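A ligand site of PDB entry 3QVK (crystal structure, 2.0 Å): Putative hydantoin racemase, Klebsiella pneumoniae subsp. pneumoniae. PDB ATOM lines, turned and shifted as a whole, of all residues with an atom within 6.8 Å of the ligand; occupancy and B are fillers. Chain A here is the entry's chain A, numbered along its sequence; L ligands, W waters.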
ATOM      1  N   ASN A   8      37.178 -17.508  19.666  1.00  0.00           N
ATOM      2  CA  ASN A   8      36.450 -17.402  20.918  1.00  0.00           C
ATOM      3  C   ASN A   8      37.305 -16.589  21.889  1.00  0.00           C
ATOM      4  O   ASN A   8      38.392 -17.041  22.251  1.00  0.00           O
ATOM      5  CB  ASN A   8      36.133 -18.795  21.479  1.00  0.00           C
ATOM      6  CG  ASN A   8      35.381 -18.745  22.811  1.00  0.00           C
ATOM      7  OD1 ASN A   8      34.788 -17.726  23.175  1.00  0.00           O
ATOM      8  ND2 ASN A   8      35.395 -19.849  23.539  1.00  0.00           N
ATOM      9  N   PRO A   9      36.845 -15.389  22.273  1.00  0.00           N
ATOM     10  CA  PRO A   9      37.622 -14.486  23.120  1.00  0.00           C
ATOM     11  C   PRO A   9      37.808 -14.981  24.558  1.00  0.00           C
ATOM     12  O   PRO A   9      38.722 -14.527  25.246  1.00  0.00           O
ATOM     13  CB  PRO A   9      36.810 -13.193  23.112  1.00  0.00           C
ATOM     14  CG  PRO A   9      35.931 -13.301  21.906  1.00  0.00           C
ATOM     15  CD  PRO A   9      35.584 -14.752  21.843  1.00  0.00           C
ATOM     16  N   ASN A  10      36.942 -15.892  24.993  1.00  0.00           N
ATOM     17  CA  ASN A  10      37.125 -16.541  26.296  1.00  0.00           C
ATOM     18  C   ASN A  10      37.901 -17.853  26.173  1.00  0.00           C
ATOM     19  O   ASN A  10      38.054 -18.385  25.062  1.00  0.00           O
ATOM     20  CB  ASN A  10      35.779 -16.716  27.034  1.00  0.00           C
ATOM     21  CG  ASN A  10      34.874 -17.769  26.399  1.00  0.00           C
ATOM     22  OD1 ASN A  10      35.267 -18.928  26.230  1.00  0.00           O
ATOM     23  ND2 ASN A  10      33.651 -17.370  26.066  1.00  0.00           N
ATOM     24  N   MET A  15      32.974 -23.880  24.891  1.00  0.00           N
ATOM     25  CA  MET A  15      32.339 -22.833  24.111  1.00  0.00           C
ATOM     26  C   MET A  15      32.991 -22.687  22.734  1.00  0.00           C
ATOM     27  O   MET A  15      32.319 -22.418  21.747  1.00  0.00           O
ATOM     28  CB  MET A  15      32.338 -21.497  24.870  1.00  0.00           C
ATOM     29  CG  MET A  15      31.329 -20.478  24.360  1.00  0.00           C
ATOM     30  SD  MET A  15      30.769 -19.318  25.627  1.00  0.00           S
ATOM     31  CE  MET A  15      29.596 -20.329  26.532  1.00  0.00           C
ATOM     32  N   ILE A  19      31.045 -22.896  19.192  1.00  0.00           N
ATOM     33  CA  ILE A  19      31.257 -21.826  18.220  1.00  0.00           C
ATOM     34  C   ILE A  19      31.824 -22.375  16.911  1.00  0.00           C
ATOM     35  O   ILE A  19      31.357 -22.005  15.825  1.00  0.00           O
ATOM     36  CB  ILE A  19      32.176 -20.718  18.817  1.00  0.00           C
ATOM     37  CG1 ILE A  19      31.411 -19.894  19.851  1.00  0.00           C
ATOM     38  CG2 ILE A  19      32.721 -19.820  17.710  1.00  0.00           C
ATOM     39  CD1 ILE A  19      32.299 -19.132  20.828  1.00  0.00           C
ATOM     40  N   VAL A  42      40.243 -15.392  30.374  1.00  0.00           N
ATOM     41  CA  VAL A  42      39.078 -15.578  31.233  1.00  0.00           C
ATOM     42  C   VAL A  42      38.142 -16.648  30.635  1.00  0.00           C
ATOM     43  O   VAL A  42      37.942 -16.675  29.425  1.00  0.00           O
ATOM     44  CB  VAL A  42      38.358 -14.208  31.473  1.00  0.00           C
ATOM     45  CG1 VAL A  42      37.686 -13.693  30.192  1.00  0.00           C
ATOM     46  CG2 VAL A  42      37.393 -14.284  32.625  1.00  0.00           C
ATOM     47  N   PRO A  43      37.593 -17.557  31.479  1.00  0.00           N
ATOM     48  CA  PRO A  43      36.718 -18.637  30.992  1.00  0.00           C
ATOM     49  C   PRO A  43      35.387 -18.163  30.400  1.00  0.00           C
ATOM     50  O   PRO A  43      34.852 -18.820  29.507  1.00  0.00           O
ATOM     51  CB  PRO A  43      36.463 -19.473  32.251  1.00  0.00           C
ATOM     52  CG  PRO A  43      37.616 -19.178  33.141  1.00  0.00           C
ATOM     53  CD  PRO A  43      37.915 -17.726  32.903  1.00  0.00           C
ATOM     54  N   SER A  44      34.854 -17.048  30.904  1.00  0.00           N
ATOM     55  CA  SER A  44      33.643 -16.444  30.355  1.00  0.00           C
ATOM     56  C   SER A  44      33.682 -14.932  30.509  1.00  0.00           C
ATOM     57  O   SER A  44      34.337 -14.415  31.417  1.00  0.00           O
ATOM     58  CB  SER A  44      32.386 -17.027  31.013  1.00  0.00           C
ATOM     59  OG  SER A  44      32.311 -16.666  32.383  1.00  0.00           O
ATOM     60  N   ILE A  45      32.994 -14.230  29.622  1.00  0.00           N
ATOM     61  CA  ILE A  45      32.993 -12.773  29.624  1.00  0.00           C
ATOM     62  C   ILE A  45      31.667 -12.238  30.147  1.00  0.00           C
ATOM     63  O   ILE A  45      30.620 -12.370  29.496  1.00  0.00           O
ATOM     64  CB  ILE A  45      33.320 -12.210  28.217  1.00  0.00           C
ATOM     65  CG1 ILE A  45      34.640 -12.789  27.699  1.00  0.00           C
ATOM     66  CG2 ILE A  45      33.386 -10.685  28.253  1.00  0.00           C
ATOM     67  CD1 ILE A  45      34.744 -12.845  26.194  1.00  0.00           C
ATOM     68  N   GLU A  46      31.711 -11.649  31.336  1.00  0.00           N
ATOM     69  CA  GLU A  46      30.515 -11.198  32.046  1.00  0.00           C
ATOM     70  C   GLU A  46      30.723  -9.811  32.658  1.00  0.00           C
ATOM     71  O   GLU A  46      30.498  -9.606  33.852  1.00  0.00           O
ATOM     72  CB  GLU A  46      30.150 -12.201  33.145  1.00  0.00           C
ATOM     73  CG  GLU A  46      29.852 -13.608  32.646  1.00  0.00           C
ATOM     74  CD  GLU A  46      29.653 -14.617  33.763  1.00  0.00           C
ATOM     75  OE1 GLU A  46      30.402 -14.557  34.760  1.00  0.00           O
ATOM     76  OE2 GLU A  46      28.759 -15.471  33.635  1.00  0.00           O
ATOM     77  N   GLU A  51      36.032  -8.229  29.510  1.00  0.00           N
ATOM     78  CA  GLU A  51      36.195  -7.789  28.123  1.00  0.00           C
ATOM     79  C   GLU A  51      37.587  -7.252  27.821  1.00  0.00           C
ATOM     80  O   GLU A  51      38.134  -7.505  26.741  1.00  0.00           O
ATOM     81  CB  GLU A  51      35.152  -6.730  27.757  1.00  0.00           C
ATOM     82  CG  GLU A  51      33.765  -7.289  27.525  1.00  0.00           C
ATOM     83  CD  GLU A  51      32.950  -6.468  26.560  1.00  0.00           C
ATOM     84  OE1 GLU A  51      33.239  -5.267  26.369  1.00  0.00           O
ATOM     85  OE2 GLU A  51      31.998  -7.041  25.981  1.00  0.00           O
ATOM     86  N   ALA A  76      34.222 -14.018  18.403  1.00  0.00           N
ATOM     87  CA  ALA A  76      33.039 -14.819  18.737  1.00  0.00           C
ATOM     88  C   ALA A  76      32.495 -14.684  20.168  1.00  0.00           C
ATOM     89  O   ALA A  76      32.163 -15.687  20.805  1.00  0.00           O
ATOM     90  CB  ALA A  76      33.281 -16.293  18.380  1.00  0.00           C
ATOM     91  N   SER A  77      32.427 -13.453  20.660  1.00  0.00           N
ATOM     92  CA  SER A  77      31.640 -13.146  21.863  1.00  0.00           C
ATOM     93  C   SER A  77      30.847 -11.857  21.660  1.00  0.00           C
ATOM     94  O   SER A  77      31.314 -10.936  20.987  1.00  0.00           O
ATOM     95  CB  SER A  77      32.520 -13.082  23.118  1.00  0.00           C
ATOM     96  OG  SER A  77      33.265 -11.890  23.177  1.00  0.00           O
ATOM     97  N   PHE A  78      29.663 -11.805  22.264  1.00  0.00           N
ATOM     98  CA  PHE A  78      28.662 -10.775  21.954  1.00  0.00           C
ATOM     99  C   PHE A  78      29.055  -9.341  22.335  1.00  0.00           C
ATOM    100  O   PHE A  78      28.332  -8.395  22.020  1.00  0.00           O
ATOM    101  CB  PHE A  78      27.312 -11.155  22.561  1.00  0.00           C
ATOM    102  CG  PHE A  78      26.141 -10.424  21.948  1.00  0.00           C
ATOM    103  CD1 PHE A  78      25.725 -10.731  20.655  1.00  0.00           C
ATOM    104  CD2 PHE A  78      25.458  -9.452  22.665  1.00  0.00           C
ATOM    105  CE1 PHE A  78      24.636 -10.060  20.093  1.00  0.00           C
ATOM    106  CE2 PHE A  78      24.375  -8.779  22.111  1.00  0.00           C
ATOM    107  CZ  PHE A  78      23.959  -9.086  20.818  1.00  0.00           C
ATOM    108  N   GLY A  79      30.188  -9.175  23.007  1.00  0.00           N
ATOM    109  CA  GLY A  79      30.702  -7.839  23.304  1.00  0.00           C
ATOM    110  C   GLY A  79      31.663  -7.322  22.255  1.00  0.00           C
ATOM    111  O   GLY A  79      32.133  -6.185  22.346  1.00  0.00           O
ATOM    112  N   ILE A  97      30.629 -10.834  16.316  1.00  0.00           N
ATOM    113  CA  ILE A  97      29.369 -11.585  16.219  1.00  0.00           C
ATOM    114  C   ILE A  97      28.132 -10.760  16.587  1.00  0.00           C
ATOM    115  O   ILE A  97      27.051 -10.999  16.062  1.00  0.00           O
ATOM    116  CB  ILE A  97      29.390 -12.938  16.981  1.00  0.00           C
ATOM    117  CG1 ILE A  97      29.604 -12.750  18.488  1.00  0.00           C
ATOM    118  CG2 ILE A  97      30.436 -13.874  16.366  1.00  0.00           C
ATOM    119  CD1 ILE A  97      29.042 -13.880  19.335  1.00  0.00           C
ATOM    120  N   THR A 116      19.963 -12.068  25.816  1.00  0.00           N
ATOM    121  CA  THR A 116      21.323 -12.360  26.261  1.00  0.00           C
ATOM    122  C   THR A 116      21.357 -13.066  27.627  1.00  0.00           C
ATOM    123  O   THR A 116      20.303 -13.478  28.141  1.00  0.00           O
ATOM    124  CB  THR A 116      22.232 -11.097  26.231  1.00  0.00           C
ATOM    125  OG1 THR A 116      23.603 -11.457  26.445  1.00  0.00           O
ATOM    126  CG2 THR A 116      21.809 -10.064  27.277  1.00  0.00           C
ATOM    127  N   THR A 117      22.546 -13.205  28.209  1.00  0.00           N
ATOM    128  CA  THR A 117      22.759 -14.016  29.407  1.00  0.00           C
ATOM    129  C   THR A 117      22.493 -13.286  30.726  1.00  0.00           C
ATOM    130  O   THR A 117      21.434 -13.467  31.333  1.00  0.00           O
ATOM    131  CB  THR A 117      24.189 -14.625  29.427  1.00  0.00           C
ATOM    132  OG1 THR A 117      25.151 -13.565  29.350  1.00  0.00           O
ATOM    133  CG2 THR A 117      24.397 -15.568  28.246  1.00  0.00           C
ATOM    134  N   LEU A 118      23.446 -12.464  31.156  1.00  0.00           N
ATOM    135  CA  LEU A 118      23.367 -11.767  32.438  1.00  0.00           C
ATOM    136  C   LEU A 118      22.890 -10.320  32.293  1.00  0.00           C
ATOM    137  O   LEU A 118      23.183  -9.672  31.287  1.00  0.00           O
ATOM    138  CB  LEU A 118      24.722 -11.795  33.151  1.00  0.00           C
ATOM    139  CG  LEU A 118      25.162 -13.064  33.890  1.00  0.00           C
ATOM    140  CD1 LEU A 118      26.573 -12.893  34.395  1.00  0.00           C
ATOM    141  CD2 LEU A 118      24.224 -13.407  35.043  1.00  0.00           C
ATOM    142  N   THR A 121      25.490  -7.536  31.448  1.00  0.00           N
ATOM    143  CA  THR A 121      26.019  -7.469  30.088  1.00  0.00           C
ATOM    144  C   THR A 121      25.138  -6.616  29.168  1.00  0.00           C
ATOM    145  O   THR A 121      25.547  -6.265  28.056  1.00  0.00           O
ATOM    146  CB  THR A 121      26.230  -8.873  29.461  1.00  0.00           C
ATOM    147  OG1 THR A 121      24.963  -9.531  29.304  1.00  0.00           O
ATOM    148  CG2 THR A 121      27.150  -9.726  30.319  1.00  0.00           C
ATOM    149  N   LEU A 122      23.936  -6.293  29.641  1.00  0.00           N
ATOM    150  CA  LEU A 122      22.974  -5.496  28.862  1.00  0.00           C
ATOM    151  C   LEU A 122      23.528  -4.122  28.474  1.00  0.00           C
ATOM    152  O   LEU A 122      23.354  -3.690  27.328  1.00  0.00           O
ATOM    153  CB  LEU A 122      21.646  -5.347  29.614  1.00  0.00           C
ATOM    154  CG  LEU A 122      20.726  -6.569  29.724  1.00  0.00           C
ATOM    155  CD1 LEU A 122      19.660  -6.343  30.788  1.00  0.00           C
ATOM    156  CD2 LEU A 122      20.087  -6.919  28.390  1.00  0.00           C
ATOM    157  N   VAL A 148      26.974 -17.045  31.712  1.00  0.00           N
ATOM    158  CA  VAL A 148      27.253 -17.390  30.317  1.00  0.00           C
ATOM    159  C   VAL A 148      27.427 -18.900  30.100  1.00  0.00           C
ATOM    160  O   VAL A 148      26.867 -19.467  29.160  1.00  0.00           O
ATOM    161  CB  VAL A 148      28.479 -16.613  29.779  1.00  0.00           C
ATOM    162  CG1 VAL A 148      28.902 -17.106  28.399  1.00  0.00           C
ATOM    163  CG2 VAL A 148      28.181 -15.113  29.723  1.00  0.00           C
ATOM    164  N   LEU A 149      28.184 -19.541  30.998  1.00  0.00           N
ATOM    165  CA  LEU A 149      28.520 -20.956  30.856  1.00  0.00           C
ATOM    166  C   LEU A 149      27.382 -21.925  31.201  1.00  0.00           C
ATOM    167  O   LEU A 149      27.540 -23.148  31.066  1.00  0.00           O
ATOM    168  CB  LEU A 149      29.790 -21.285  31.664  1.00  0.00           C
ATOM    169  CG  LEU A 149      31.074 -20.551  31.273  1.00  0.00           C
ATOM    170  CD1 LEU A 149      32.186 -20.838  32.267  1.00  0.00           C
ATOM    171  CD2 LEU A 149      31.513 -20.889  29.848  1.00  0.00           C
ATOM    172  N   LEU A 151      24.862 -22.243  29.463  1.00  0.00           N
ATOM    173  CA  LEU A 151      24.534 -22.793  28.138  1.00  0.00           C
ATOM    174  C   LEU A 151      25.330 -24.057  27.817  1.00  0.00           C
ATOM    175  O   LEU A 151      24.957 -24.819  26.915  1.00  0.00           O
ATOM    176  CB  LEU A 151      24.788 -21.736  27.058  1.00  0.00           C
ATOM    177  CG  LEU A 151      23.867 -20.506  27.028  1.00  0.00           C
ATOM    178  CD1 LEU A 151      24.577 -19.325  26.378  1.00  0.00           C
ATOM    179  CD2 LEU A 151      22.551 -20.813  26.319  1.00  0.00           C
ATOM    180  N   GLY A 181      22.116 -13.087  22.110  1.00  0.00           N
ATOM    181  CA  GLY A 181      23.190 -12.287  22.689  1.00  0.00           C
ATOM    182  C   GLY A 181      24.331 -13.045  23.330  1.00  0.00           C
ATOM    183  O   GLY A 181      24.878 -12.610  24.342  1.00  0.00           O
ATOM    184  N   SER A 182      24.696 -14.181  22.743  1.00  0.00           N
ATOM    185  CA  SER A 182      25.823 -14.987  23.235  1.00  0.00           C
ATOM    186  C   SER A 182      26.347 -15.942  22.162  1.00  0.00           C
ATOM    187  O   SER A 182      25.579 -16.414  21.314  1.00  0.00           O
ATOM    188  CB  SER A 182      25.431 -15.771  24.480  1.00  0.00           C
ATOM    189  OG  SER A 182      26.564 -16.412  25.065  1.00  0.00           O
ATOM    190  N   GLY A 183      27.639 -16.220  22.207  1.00  0.00           N
ATOM    191  CA  GLY A 183      28.263 -17.210  21.337  1.00  0.00           C
ATOM    192  C   GLY A 183      27.875 -18.632  21.684  1.00  0.00           C
ATOM    193  O   GLY A 183      28.015 -19.545  20.867  1.00  0.00           O
ATOM    194  N   GLY A 184      27.373 -18.819  22.904  1.00  0.00           N
ATOM    195  CA  GLY A 184      26.923 -20.131  23.379  1.00  0.00           C
ATOM    196  C   GLY A 184      25.558 -20.540  22.854  1.00  0.00           C
ATOM    197  O   GLY A 184      25.213 -21.728  22.870  1.00  0.00           O
ATOM    198  N   MET A 185      24.788 -19.556  22.399  1.00  0.00           N
ATOM    199  CA  MET A 185      23.443 -19.796  21.848  1.00  0.00           C
ATOM    200  C   MET A 185      23.505 -20.095  20.345  1.00  0.00           C
ATOM    201  O   MET A 185      22.463 -20.263  19.701  1.00  0.00           O
ATOM    202  CB  MET A 185      22.542 -18.583  22.092  1.00  0.00           C
ATOM    203  CG  MET A 185      22.351 -18.220  23.548  1.00  0.00           C
ATOM    204  SD  MET A 185      21.408 -16.696  23.761  1.00  0.00           S
ATOM    205  CE  MET A 185      21.752 -16.337  25.489  1.00  0.00           C
HETATM  206  C1  LIG L   1      29.576 -13.383  26.038  1.00  0.00           C
HETATM  207  C2  LIG L   1      29.742 -14.251  24.971  1.00  0.00           C
HETATM  208  O1  LIG L   1      29.144 -14.214  23.897  1.00  0.00           O
HETATM  209  N1  LIG L   1      30.678 -15.132  25.302  1.00  0.00           N
HETATM  210  C3  LIG L   1      31.064 -14.814  26.538  1.00  0.00           C
HETATM  211  O2  LIG L   1      31.927 -15.423  27.175  1.00  0.00           O
HETATM  212  N2  LIG L   1      30.400 -13.751  27.007  1.00  0.00           N
HETATM  213  N3  LIG L   1      28.734 -12.348  26.103  1.00  0.00           N
HETATM  214  C4  LIG L   1      27.460 -12.475  26.487  1.00  0.00           C
HETATM  215  N4  LIG L   1      27.017 -13.683  26.803  1.00  0.00           N
HETATM  216  O3  LIG L   1      26.721 -11.489  26.549  1.00  0.00           O
HETATM  217  O   HOH W   1      32.370 -16.516  23.492  1.00  0.00           O
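An oxygen (O2) of the ligand lies within hydrogen-bond range of the side-chain amide nitrogen (ND2) of Asn 10 (2.8 Å). The backbone NH of Ile 45 is in hydrogen-bond range of an oxygen (O2) of the ligand. The backbone NH of Phe 78 sits at hydrogen-bond distance from an oxygen (O1) of the ligand (3.0 Å). The backbone NH (N) of Gly 183 sits at hydrogen-bond distance from an oxygen (O1) of the ligand (3.0 Å). The backbone carbonyl oxygen of Gly 181 lies close to a nitrogen (N4) of the ligand (3.4 Å). The side-chain hydroxyl (OG1) of Thr 116 is in hydrogen-bond range of an oxygen (O3) of the ligand (3.1 Å). N4 of the ligand is in hydrogen-bond range of OG1 of Thr 117 (3.2 Å). The side-chain hydroxyl of Ser 182 lies within hydrogen-bond range of a nitrogen (N4) of the ligand, 3.3 Å away.
Water W1 lies within hydrogen-bond range of OD1 of Asn 8 (2.7 Å), O of Ala 76 (2.8 Å), N1 of the ligand (2.8 Å) and ND2 of Asn 10 (3.0 Å).
SD of Met 15 is in hydrogen-bond range of ND2 of Asn 10, at 3.5 Å. OD1 of Asn 10 sits close to O of Pro 43, at 3.3 Å. The side-chain amide nitrogen (ND2) of Asn 8 lies within hydrogen-bond range of the side-chain amide oxygen (OD1) of Asn 10 (2.8 Å). The backbone carbonyl oxygen (O) of Gly 181 lies within hydrogen-bond range of the side-chain hydroxyl (OG1) of Thr 116, 2.7 Å away. The side-chain hydroxyl of Ser 182 sits close to the backbone NH of Gly 184 (3.3 Å). N of Val 148 sits at hydrogen-bond distance from OE2 of Glu 46. OG1 of Thr 121 sits at hydrogen-bond distance from O of Leu 118 (2.7 Å).
Ser 44 touches the ligand (CA to O2, 3.8 Å). Ser 77 touches the ligand. OG1 of Thr 121 touches O3 of the ligand, 3.8 Å away. Val 148 touches the ligand (CG2 to N4, 3.5 Å). Hydrophobic or aromatic side chains within 4 Å of the ligand: Ile 45, Phe 78 and Val 148. 12 residues have an atom within 4 Å of the ligand: Asn 10, Ser 44, Ile 45, Ser 77, Phe 78, Thr 116, Thr 117, Thr 121, Val 148, Gly 181, Ser 182 and Gly 183.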
